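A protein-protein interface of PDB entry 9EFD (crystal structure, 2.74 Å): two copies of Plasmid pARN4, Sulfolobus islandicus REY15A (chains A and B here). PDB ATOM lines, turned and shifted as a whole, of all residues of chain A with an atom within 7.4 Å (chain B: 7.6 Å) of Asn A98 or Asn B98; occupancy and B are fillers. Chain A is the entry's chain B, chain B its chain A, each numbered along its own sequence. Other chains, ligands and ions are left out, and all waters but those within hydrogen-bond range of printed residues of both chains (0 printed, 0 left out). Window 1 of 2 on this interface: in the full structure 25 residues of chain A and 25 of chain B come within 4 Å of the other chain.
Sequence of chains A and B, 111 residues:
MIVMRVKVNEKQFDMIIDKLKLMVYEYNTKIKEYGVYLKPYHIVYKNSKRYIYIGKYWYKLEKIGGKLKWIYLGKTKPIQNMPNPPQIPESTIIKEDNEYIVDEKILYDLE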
ATOM      1  N   VAL A   8      13.533  -0.188   1.179  1.00  0.00           N
ATOM      2  CA  VAL A   8      13.439  -1.311   2.100  1.00  0.00           C
ATOM      3  C   VAL A   8      12.256  -1.085   3.030  1.00  0.00           C
ATOM      4  O   VAL A   8      11.834   0.048   3.275  1.00  0.00           O
ATOM      5  CB  VAL A   8      14.736  -1.506   2.916  1.00  0.00           C
ATOM      6  CG1 VAL A   8      15.869  -1.960   2.009  1.00  0.00           C
ATOM      7  CG2 VAL A   8      15.104  -0.220   3.638  1.00  0.00           C
ATOM      8  N   ASN A   9      11.723  -2.186   3.553  1.00  0.00           N
ATOM      9  CA  ASN A   9      10.549  -2.123   4.408  1.00  0.00           C
ATOM     10  C   ASN A   9      10.955  -1.796   5.845  1.00  0.00           C
ATOM     11  O   ASN A   9      12.134  -1.610   6.162  1.00  0.00           O
ATOM     12  CB  ASN A   9       9.763  -3.431   4.327  1.00  0.00           C
ATOM     13  CG  ASN A   9      10.561  -4.630   4.811  1.00  0.00           C
ATOM     14  OD1 ASN A   9      11.397  -4.521   5.708  1.00  0.00           O
ATOM     15  ND2 ASN A   9      10.302  -5.787   4.213  1.00  0.00           N
ATOM     16  N   GLU A  10       9.958  -1.726   6.729  1.00  0.00           N
ATOM     17  CA  GLU A  10      10.230  -1.368   8.118  1.00  0.00           C
ATOM     18  C   GLU A  10      11.132  -2.398   8.782  1.00  0.00           C
ATOM     19  O   GLU A  10      12.015  -2.046   9.574  1.00  0.00           O
ATOM     20  CB  GLU A  10       8.916  -1.224   8.889  1.00  0.00           C
ATOM     21  CG  GLU A  10       9.064  -1.320  10.400  1.00  0.00           C
ATOM     22  CD  GLU A  10       9.633  -0.054  11.012  1.00  0.00           C
ATOM     23  OE1 GLU A  10       9.994   0.867  10.251  1.00  0.00           O
ATOM     24  OE2 GLU A  10       9.717   0.020  12.257  1.00  0.00           O
ATOM     25  N   LYS A  11      10.922  -3.679   8.474  1.00  0.00           N
ATOM     26  CA  LYS A  11      11.728  -4.728   9.087  1.00  0.00           C
ATOM     27  C   LYS A  11      13.193  -4.598   8.696  1.00  0.00           C
ATOM     28  O   LYS A  11      14.085  -4.765   9.536  1.00  0.00           O
ATOM     29  CB  LYS A  11      11.184  -6.097   8.686  1.00  0.00           C
ATOM     30  CG  LYS A  11      10.134  -6.633   9.635  1.00  0.00           C
ATOM     31  CD  LYS A  11       9.136  -7.504   8.902  1.00  0.00           C
ATOM     32  CE  LYS A  11       8.528  -8.516   9.839  1.00  0.00           C
ATOM     33  NZ  LYS A  11       9.512  -9.584  10.102  1.00  0.00           N
ATOM     34  N   GLN A  12      13.463  -4.299   7.423  1.00  0.00           N
ATOM     35  CA  GLN A  12      14.838  -4.049   7.002  1.00  0.00           C
ATOM     36  C   GLN A  12      15.397  -2.786   7.647  1.00  0.00           C
ATOM     37  O   GLN A  12      16.580  -2.737   8.003  1.00  0.00           O
ATOM     38  CB  GLN A  12      14.911  -3.959   5.477  1.00  0.00           C
ATOM     39  CG  GLN A  12      14.395  -5.199   4.766  1.00  0.00           C
ATOM     40  CD  GLN A  12      14.223  -4.990   3.276  1.00  0.00           C
ATOM     41  OE1 GLN A  12      13.262  -4.360   2.832  1.00  0.00           O
ATOM     42  NE2 GLN A  12      15.153  -5.522   2.491  1.00  0.00           N
ATOM     43  N   PHE A  13      14.567  -1.751   7.797  1.00  0.00           N
ATOM     44  CA  PHE A  13      15.054  -0.501   8.373  1.00  0.00           C
ATOM     45  C   PHE A  13      15.464  -0.678   9.831  1.00  0.00           C
ATOM     46  O   PHE A  13      16.515  -0.179  10.249  1.00  0.00           O
ATOM     47  CB  PHE A  13      13.991   0.591   8.248  1.00  0.00           C
ATOM     48  CG  PHE A  13      14.279   1.807   9.081  1.00  0.00           C
ATOM     49  CD1 PHE A  13      15.161   2.775   8.631  1.00  0.00           C
ATOM     50  CD2 PHE A  13      13.675   1.980  10.316  1.00  0.00           C
ATOM     51  CE1 PHE A  13      15.432   3.893   9.394  1.00  0.00           C
ATOM     52  CE2 PHE A  13      13.943   3.096  11.083  1.00  0.00           C
ATOM     53  CZ  PHE A  13      14.823   4.052  10.624  1.00  0.00           C
ATOM     54  N   ASP A  14      14.648  -1.382  10.622  1.00  0.00           N
ATOM     55  CA  ASP A  14      15.050  -1.703  11.986  1.00  0.00           C
ATOM     56  C   ASP A  14      16.374  -2.451  12.012  1.00  0.00           C
ATOM     57  O   ASP A  14      17.147  -2.319  12.969  1.00  0.00           O
ATOM     58  CB  ASP A  14      13.962  -2.524  12.683  1.00  0.00           C
ATOM     59  CG  ASP A  14      12.568  -1.958  12.464  1.00  0.00           C
ATOM     60  OD1 ASP A  14      12.454  -0.838  11.923  1.00  0.00           O
ATOM     61  OD2 ASP A  14      11.586  -2.635  12.835  1.00  0.00           O
ATOM     62  N   ARG A  50       9.542  11.996   7.923  1.00  0.00           N
ATOM     63  CA  ARG A  50      10.599  11.537   8.818  1.00  0.00           C
ATOM     64  C   ARG A  50      11.910  11.479   8.044  1.00  0.00           C
ATOM     65  O   ARG A  50      12.079  10.637   7.155  1.00  0.00           O
ATOM     66  CB  ARG A  50      10.246  10.176   9.410  1.00  0.00           C
ATOM     67  CG  ARG A  50      11.029   9.825  10.665  1.00  0.00           C
ATOM     68  CD  ARG A  50      10.448   8.606  11.362  1.00  0.00           C
ATOM     69  NE  ARG A  50       9.077   8.828  11.805  1.00  0.00           N
ATOM     70  CZ  ARG A  50       8.226   7.864  12.125  1.00  0.00           C
ATOM     71  NH1 ARG A  50       8.575   6.588  12.068  1.00  0.00           N
ATOM     72  NH2 ARG A  50       6.995   8.185  12.513  1.00  0.00           N
ATOM     73  N   LYS A  95      11.833   8.404   5.204  1.00  0.00           N
ATOM     74  CA  LYS A  95      10.579   7.670   5.309  1.00  0.00           C
ATOM     75  C   LYS A  95       9.694   7.968   4.106  1.00  0.00           C
ATOM     76  O   LYS A  95       9.471   9.131   3.757  1.00  0.00           O
ATOM     77  CB  LYS A  95       9.857   8.035   6.603  1.00  0.00           C
ATOM     78  CG  LYS A  95       9.896   6.947   7.661  1.00  0.00           C
ATOM     79  CD  LYS A  95       8.797   5.921   7.439  1.00  0.00           C
ATOM     80  CE  LYS A  95       7.455   6.435   7.931  1.00  0.00           C
ATOM     81  NZ  LYS A  95       6.422   5.364   7.941  1.00  0.00           N
ATOM     82  N   GLU A  96       9.189   6.914   3.474  1.00  0.00           N
ATOM     83  CA  GLU A  96       8.054   7.052   2.574  1.00  0.00           C
ATOM     84  C   GLU A  96       6.796   7.434   3.345  1.00  0.00           C
ATOM     85  O   GLU A  96       6.624   7.085   4.516  1.00  0.00           O
ATOM     86  CB  GLU A  96       7.823   5.753   1.804  1.00  0.00           C
ATOM     87  CG  GLU A  96       9.016   5.315   0.973  1.00  0.00           C
ATOM     88  CD  GLU A  96       9.156   6.118  -0.303  1.00  0.00           C
ATOM     89  OE1 GLU A  96       9.686   7.248  -0.239  1.00  0.00           O
ATOM     90  OE2 GLU A  96       8.738   5.622  -1.369  1.00  0.00           O
ATOM     91  N   ASP A  97       5.909   8.163   2.672  1.00  0.00           N
ATOM     92  CA  ASP A  97       4.593   8.436   3.230  1.00  0.00           C
ATOM     93  C   ASP A  97       3.836   7.136   3.471  1.00  0.00           C
ATOM     94  O   ASP A  97       3.873   6.214   2.652  1.00  0.00           O
ATOM     95  CB  ASP A  97       3.795   9.345   2.294  1.00  0.00           C
ATOM     96  CG  ASP A  97       4.646  10.439   1.678  1.00  0.00           C
ATOM     97  OD1 ASP A  97       4.939  10.355   0.467  1.00  0.00           O
ATOM     98  OD2 ASP A  97       5.022  11.381   2.405  1.00  0.00           O
ATOM     99  N   ASN A  98       3.145   7.070   4.606  1.00  0.00           N
ATOM    100  CA  ASN A  98       2.329   5.902   4.908  1.00  0.00           C
ATOM    101  C   ASN A  98       1.196   5.771   3.899  1.00  0.00           C
ATOM    102  O   ASN A  98       0.628   6.767   3.441  1.00  0.00           O
ATOM    103  CB  ASN A  98       1.768   5.999   6.325  1.00  0.00           C
ATOM    104  CG  ASN A  98       2.842   6.264   7.361  1.00  0.00           C
ATOM    105  OD1 ASN A  98       3.300   5.349   8.045  1.00  0.00           O
ATOM    106  ND2 ASN A  98       3.249   7.523   7.482  1.00  0.00           N
ATOM    107  N   GLU A  99       0.868   4.530   3.551  1.00  0.00           N
ATOM    108  CA  GLU A  99      -0.185   4.238   2.591  1.00  0.00           C
ATOM    109  C   GLU A  99      -1.085   3.142   3.141  1.00  0.00           C
ATOM    110  O   GLU A  99      -0.613   2.214   3.805  1.00  0.00           O
ATOM    111  CB  GLU A  99       0.397   3.816   1.237  1.00  0.00           C
ATOM    112  CG  GLU A  99       0.938   4.975   0.413  1.00  0.00           C
ATOM    113  CD  GLU A  99       0.297   5.067  -0.959  1.00  0.00           C
ATOM    114  OE1 GLU A  99      -0.009   6.197  -1.397  1.00  0.00           O
ATOM    115  OE2 GLU A  99       0.104   4.012  -1.599  1.00  0.00           O
ATOM    116  N   TYR A 100      -2.381   3.259   2.862  1.00  0.00           N
ATOM    117  CA  TYR A 100      -3.395   2.400   3.458  1.00  0.00           C
ATOM    118  C   TYR A 100      -4.223   1.772   2.348  1.00  0.00           C
ATOM    119  O   TYR A 100      -4.689   2.475   1.445  1.00  0.00           O
ATOM    120  CB  TYR A 100      -4.296   3.187   4.414  1.00  0.00           C
ATOM    121  CG  TYR A 100      -3.556   3.817   5.572  1.00  0.00           C
ATOM    122  CD1 TYR A 100      -2.822   4.983   5.401  1.00  0.00           C
ATOM    123  CD2 TYR A 100      -3.594   3.248   6.838  1.00  0.00           C
ATOM    124  CE1 TYR A 100      -2.145   5.563   6.456  1.00  0.00           C
ATOM    125  CE2 TYR A 100      -2.921   3.820   7.899  1.00  0.00           C
ATOM    126  CZ  TYR A 100      -2.199   4.978   7.703  1.00  0.00           C
ATOM    127  OH  TYR A 100      -1.527   5.550   8.759  1.00  0.00           O
ATOM    128  N   VAL B   8      -4.528   4.597  -0.375  1.00  0.00           N
ATOM    129  CA  VAL B   8      -4.549   6.014  -0.043  1.00  0.00           C
ATOM    130  C   VAL B   8      -3.415   6.308   0.931  1.00  0.00           C
ATOM    131  O   VAL B   8      -2.900   5.419   1.612  1.00  0.00           O
ATOM    132  CB  VAL B   8      -5.902   6.456   0.556  1.00  0.00           C
ATOM    133  CG1 VAL B   8      -7.043   6.076  -0.374  1.00  0.00           C
ATOM    134  CG2 VAL B   8      -6.101   5.840   1.933  1.00  0.00           C
ATOM    135  N   ASN B   9      -3.027   7.581   0.984  1.00  0.00           N
ATOM    136  CA  ASN B   9      -1.949   8.017   1.857  1.00  0.00           C
ATOM    137  C   ASN B   9      -2.512   8.508   3.189  1.00  0.00           C
ATOM    138  O   ASN B   9      -3.724   8.508   3.423  1.00  0.00           O
ATOM    139  CB  ASN B   9      -1.120   9.103   1.174  1.00  0.00           C
ATOM    140  CG  ASN B   9      -1.970  10.249   0.665  1.00  0.00           C
ATOM    141  OD1 ASN B   9      -2.615  10.952   1.443  1.00  0.00           O
ATOM    142  ND2 ASN B   9      -1.976  10.442  -0.649  1.00  0.00           N
ATOM    143  N   GLU B  10      -1.615   8.937   4.080  1.00  0.00           N
ATOM    144  CA  GLU B  10      -2.019   9.235   5.451  1.00  0.00           C
ATOM    145  C   GLU B  10      -3.024  10.379   5.493  1.00  0.00           C
ATOM    146  O   GLU B  10      -3.975  10.351   6.283  1.00  0.00           O
ATOM    147  CB  GLU B  10      -0.793   9.568   6.302  1.00  0.00           C
ATOM    148  CG  GLU B  10      -1.124  10.080   7.696  1.00  0.00           C
ATOM    149  CD  GLU B  10      -1.149   8.976   8.735  1.00  0.00           C
ATOM    150  OE1 GLU B  10      -0.460   7.953   8.535  1.00  0.00           O
ATOM    151  OE2 GLU B  10      -1.856   9.131   9.752  1.00  0.00           O
ATOM    152  N   LYS B  11      -2.828  11.397   4.655  1.00  0.00           N
ATOM    153  CA  LYS B  11      -3.711  12.558   4.680  1.00  0.00           C
ATOM    154  C   LYS B  11      -5.146  12.162   4.358  1.00  0.00           C
ATOM    155  O   LYS B  11      -6.087  12.572   5.048  1.00  0.00           O
ATOM    156  CB  LYS B  11      -3.206  13.618   3.699  1.00  0.00           C
ATOM    157  CG  LYS B  11      -3.341  15.046   4.197  1.00  0.00           C
ATOM    158  CD  LYS B  11      -4.563  15.723   3.597  1.00  0.00           C
ATOM    159  CE  LYS B  11      -4.692  17.157   4.085  1.00  0.00           C
ATOM    160  NZ  LYS B  11      -4.771  17.233   5.569  1.00  0.00           N
ATOM    161  N   GLN B  12      -5.335  11.356   3.311  1.00  0.00           N
ATOM    162  CA  GLN B  12      -6.669  10.855   2.998  1.00  0.00           C
ATOM    163  C   GLN B  12      -7.178   9.910   4.079  1.00  0.00           C
ATOM    164  O   GLN B  12      -8.347   9.987   4.478  1.00  0.00           O
ATOM    165  CB  GLN B  12      -6.664  10.162   1.635  1.00  0.00           C
ATOM    166  CG  GLN B  12      -5.511  10.573   0.737  1.00  0.00           C
ATOM    167  CD  GLN B  12      -5.724  10.161  -0.706  1.00  0.00           C
ATOM    168  OE1 GLN B  12      -6.694  10.571  -1.344  1.00  0.00           O
ATOM    169  NE2 GLN B  12      -4.816   9.344  -1.229  1.00  0.00           N
ATOM    170  N   PHE B  13      -6.319   9.012   4.567  1.00  0.00           N
ATOM    171  CA  PHE B  13      -6.728   8.108   5.637  1.00  0.00           C
ATOM    172  C   PHE B  13      -7.079   8.877   6.904  1.00  0.00           C
ATOM    173  O   PHE B  13      -8.059   8.556   7.585  1.00  0.00           O
ATOM    174  CB  PHE B  13      -5.624   7.088   5.918  1.00  0.00           C
ATOM    175  CG  PHE B  13      -5.805   6.341   7.208  1.00  0.00           C
ATOM    176  CD1 PHE B  13      -6.706   5.293   7.297  1.00  0.00           C
ATOM    177  CD2 PHE B  13      -5.074   6.687   8.333  1.00  0.00           C
ATOM    178  CE1 PHE B  13      -6.876   4.603   8.483  1.00  0.00           C
ATOM    179  CE2 PHE B  13      -5.239   6.001   9.522  1.00  0.00           C
ATOM    180  CZ  PHE B  13      -6.140   4.958   9.597  1.00  0.00           C
ATOM    181  N   SER B  48       2.157  -7.355  13.088  1.00  0.00           N
ATOM    182  CA  SER B  48       2.969  -6.142  13.057  1.00  0.00           C
ATOM    183  C   SER B  48       2.556  -5.195  11.934  1.00  0.00           C
ATOM    184  O   SER B  48       3.315  -4.291  11.570  1.00  0.00           O
ATOM    185  CB  SER B  48       4.461  -6.479  12.941  1.00  0.00           C
ATOM    186  OG  SER B  48       5.078  -6.517  14.215  1.00  0.00           O
ATOM    187  N   ARG B  50      -0.704  -2.431  11.260  1.00  0.00           N
ATOM    188  CA  ARG B  50      -1.780  -1.713  11.939  1.00  0.00           C
ATOM    189  C   ARG B  50      -3.060  -1.897  11.134  1.00  0.00           C
ATOM    190  O   ARG B  50      -3.284  -1.212  10.133  1.00  0.00           O
ATOM    191  CB  ARG B  50      -1.425  -0.239  12.104  1.00  0.00           C
ATOM    192  CG  ARG B  50      -1.818   0.343  13.453  1.00  0.00           C
ATOM    193  CD  ARG B  50      -1.046   1.619  13.758  1.00  0.00           C
ATOM    194  NE  ARG B  50      -1.370   2.700  12.835  1.00  0.00           N
ATOM    195  CZ  ARG B  50      -0.525   3.659  12.480  1.00  0.00           C
ATOM    196  NH1 ARG B  50       0.710   3.700  12.951  1.00  0.00           N
ATOM    197  NH2 ARG B  50      -0.931   4.599  11.631  1.00  0.00           N
ATOM    198  N   LYS B  95      -3.095  -0.901   6.930  1.00  0.00           N
ATOM    199  CA  LYS B  95      -1.916  -0.078   6.701  1.00  0.00           C
ATOM    200  C   LYS B  95      -0.779  -0.931   6.153  1.00  0.00           C
ATOM    201  O   LYS B  95      -0.455  -1.984   6.710  1.00  0.00           O
ATOM    202  CB  LYS B  95      -1.486   0.611   7.995  1.00  0.00           C
ATOM    203  CG  LYS B  95      -0.229   1.454   7.858  1.00  0.00           C
ATOM    204  CD  LYS B  95      -0.087   2.431   9.012  1.00  0.00           C
ATOM    205  CE  LYS B  95       1.262   3.131   8.977  1.00  0.00           C
ATOM    206  NZ  LYS B  95       2.381   2.167   8.788  1.00  0.00           N
ATOM    207  N   GLU B  96      -0.176  -0.471   5.060  1.00  0.00           N
ATOM    208  CA  GLU B  96       0.952  -1.175   4.474  1.00  0.00           C
ATOM    209  C   GLU B  96       2.196  -1.008   5.347  1.00  0.00           C
ATOM    210  O   GLU B  96       2.262  -0.154   6.235  1.00  0.00           O
ATOM    211  CB  GLU B  96       1.223  -0.670   3.058  1.00  0.00           C
ATOM    212  CG  GLU B  96       0.069  -0.888   2.092  1.00  0.00           C
ATOM    213  CD  GLU B  96       0.538  -1.193   0.683  1.00  0.00           C
ATOM    214  OE1 GLU B  96       0.428  -2.363   0.259  1.00  0.00           O
ATOM    215  OE2 GLU B  96       1.014  -0.263  -0.002  1.00  0.00           O
ATOM    216  N   ASP B  97       3.194  -1.848   5.083  1.00  0.00           N
ATOM    217  CA  ASP B  97       4.481  -1.704   5.747  1.00  0.00           C
ATOM    218  C   ASP B  97       5.094  -0.346   5.430  1.00  0.00           C
ATOM    219  O   ASP B  97       5.009   0.145   4.301  1.00  0.00           O
ATOM    220  CB  ASP B  97       5.428  -2.825   5.316  1.00  0.00           C
ATOM    221  CG  ASP B  97       5.121  -4.144   5.998  1.00  0.00           C
ATOM    222  OD1 ASP B  97       5.083  -5.180   5.302  1.00  0.00           O
ATOM    223  OD2 ASP B  97       4.916  -4.144   7.230  1.00  0.00           O
ATOM    224  N   ASN B  98       5.714   0.262   6.439  1.00  0.00           N
ATOM    225  CA  ASN B  98       6.510   1.460   6.208  1.00  0.00           C
ATOM    226  C   ASN B  98       7.688   1.147   5.292  1.00  0.00           C
ATOM    227  O   ASN B  98       8.269   0.059   5.347  1.00  0.00           O
ATOM    228  CB  ASN B  98       7.013   2.028   7.536  1.00  0.00           C
ATOM    229  CG  ASN B  98       5.893   2.260   8.532  1.00  0.00           C
ATOM    230  OD1 ASN B  98       4.785   2.645   8.159  1.00  0.00           O
ATOM    231  ND2 ASN B  98       6.179   2.028   9.808  1.00  0.00           N
ATOM    232  N   GLU B  99       8.034   2.110   4.443  1.00  0.00           N
ATOM    233  CA  GLU B  99       9.070   1.931   3.437  1.00  0.00           C
ATOM    234  C   GLU B  99      10.043   3.098   3.488  1.00  0.00           C
ATOM    235  O   GLU B  99       9.658   4.239   3.761  1.00  0.00           O
ATOM    236  CB  GLU B  99       8.472   1.811   2.029  1.00  0.00           C
ATOM    237  CG  GLU B  99       7.668   0.540   1.806  1.00  0.00           C
ATOM    238  CD  GLU B  99       8.394  -0.462   0.932  1.00  0.00           C
ATOM    239  OE1 GLU B  99       9.247  -0.040   0.123  1.00  0.00           O
ATOM    240  OE2 GLU B  99       8.113  -1.673   1.055  1.00  0.00           O
ATOM    241  N   TYR B 100      11.313   2.798   3.224  1.00  0.00           N
ATOM    242  CA  TYR B 100      12.407   3.731   3.454  1.00  0.00           C
ATOM    243  C   TYR B 100      13.292   3.767   2.220  1.00  0.00           C
ATOM    244  O   TYR B 100      13.651   2.717   1.678  1.00  0.00           O
ATOM    245  CB  TYR B 100      13.227   3.331   4.686  1.00  0.00           C
ATOM    246  CG  TYR B 100      12.423   3.264   5.965  1.00  0.00           C
ATOM    247  CD1 TYR B 100      11.599   2.180   6.238  1.00  0.00           C
ATOM    248  CD2 TYR B 100      12.487   4.288   6.901  1.00  0.00           C
ATOM    249  CE1 TYR B 100      10.863   2.117   7.406  1.00  0.00           C
ATOM    250  CE2 TYR B 100      11.755   4.234   8.072  1.00  0.00           C
ATOM    251  CZ  TYR B 100      10.944   3.146   8.320  1.00  0.00           C
ATOM    252  OH  TYR B 100      10.214   3.089   9.485  1.00  0.00           O
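O of Val B8 sits at hydrogen-bond distance from N of Tyr A100. The backbone carbonyl oxygen of Asn A98 sits at hydrogen-bond distance from the backbone NH of Glu B10, 3.2 Å away. OE1 of Glu B10 is in hydrogen-bond range of OH of Tyr A100 (2.6 Å). The guanidinium group of Arg B50 sits at hydrogen-bond distance from the side-chain hydroxyl of Tyr A100 (3.1 Å). The side-chain amide oxygen (OD1) of Asn A98 lies close to the side-chain amino group (NZ) of Lys B95, at 3.4 Å. O of Glu A99 sits at hydrogen-bond distance from N of Glu B96, 3.0 Å away. The backbone carbonyl oxygen (O) of Asn B98 lies within hydrogen-bond range of the backbone NH (N) of Glu A10 (2.8 Å). NZ of Lys A95 lies within hydrogen-bond range of OD1 of Asn B98. OD1 of Asn B98 sits close to OD1 of Asn A98 (3.1 Å). N of Glu A96 sits at hydrogen-bond distance from O of Glu B99 (2.7 Å). N of Tyr B100 lies within hydrogen-bond range of O of Val A8 (2.8 Å). The side-chain hydroxyl (OH) of Tyr B100 lies close to the side-chain carboxylate (OE1) of Glu A10, 2.4 Å away.
N of Lys B11 sits at hydrogen-bond distance from OD1 of Asn B9 (3.2 Å). The backbone carbonyl oxygen (O) of Arg B50 sits at hydrogen-bond distance from the backbone NH (N) of Lys B95. NZ of Lys B95 sits at hydrogen-bond distance from OD1 of Asn B98 (2.5 Å). The side-chain amide oxygen of Asn A9 lies within hydrogen-bond range of the backbone NH of Lys A11, 2.9 Å away. The backbone NH of Gln A12 is in hydrogen-bond range of the side-chain amide oxygen of Asn A9, 2.7 Å away. NZ of Lys A95 is in hydrogen-bond range of OD1 of Asn A98 (3.1 Å).
Among the printed residues, merely in contact across the chains: Val A8 with Glu B99 (3.3 Å), Asn A9 with Asn B98 (3.3 Å), Asn A9 with Tyr B100 (3.8 Å), Phe A13 with Tyr B100 (3.5 Å), Lys A95 with Glu B99 (3.7 Å), Lys A95 with Tyr B100 (3.3 Å), Asn A98 with Asn B9 (3.3 Å), Glu A99 with Val B8 (3.1 Å), Glu A99 with Lys B95 (3.9 Å), Tyr A100 with Phe B13 (3.4 Å) and Tyr A100 with Lys B95 (3.3 Å).
Printed residues of chain B within 4 Å of Phe A13: Tyr B100. Asp A97 touches none of the printed residues of chain B. Asn A98 touches four residues of chain B. Gln B12 touches none of the printed residues of chain A. Printed residues of chain A within 4 Å of Tyr B100: Val A8, Asn A9, Glu A10, Phe A13 and Lys A95. The nearest residue of chain B that does not touch Asn A98 is Val B8 (4.2 Å). The nearest residue of chain A that does not touch Asn B98 is Val A8 (4.1 Å). The nearest printed residue of chain A that does not touch Glu B10 is Glu A99 (5.1 Å).
Of the 14 printed residues of chain A, 9 touch a printed residue of chain B. Along chain A the printed residues that touch a printed residue of chain B span positions 8 to 100. Of the 14 printed residues of chain B, 10 touch a printed residue of chain A.
Val A8 touches Tyr B100, and with the chains exchanged Tyr A100 touches Val B8. Lys A95 touches Tyr B100, and with the chains exchanged Tyr A100 touches Lys B95. Glu A96 touches Glu B99, and with the chains exchanged Glu A99 touches Glu B96. Tyr A100 touches Arg B50, but with the chains exchanged Arg A50 does not touch Tyr B100 (4.6 Å). Of the 23 pairs that touch across the chains among the printed residues, 21 have their exchanged pair printed and touching as well.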
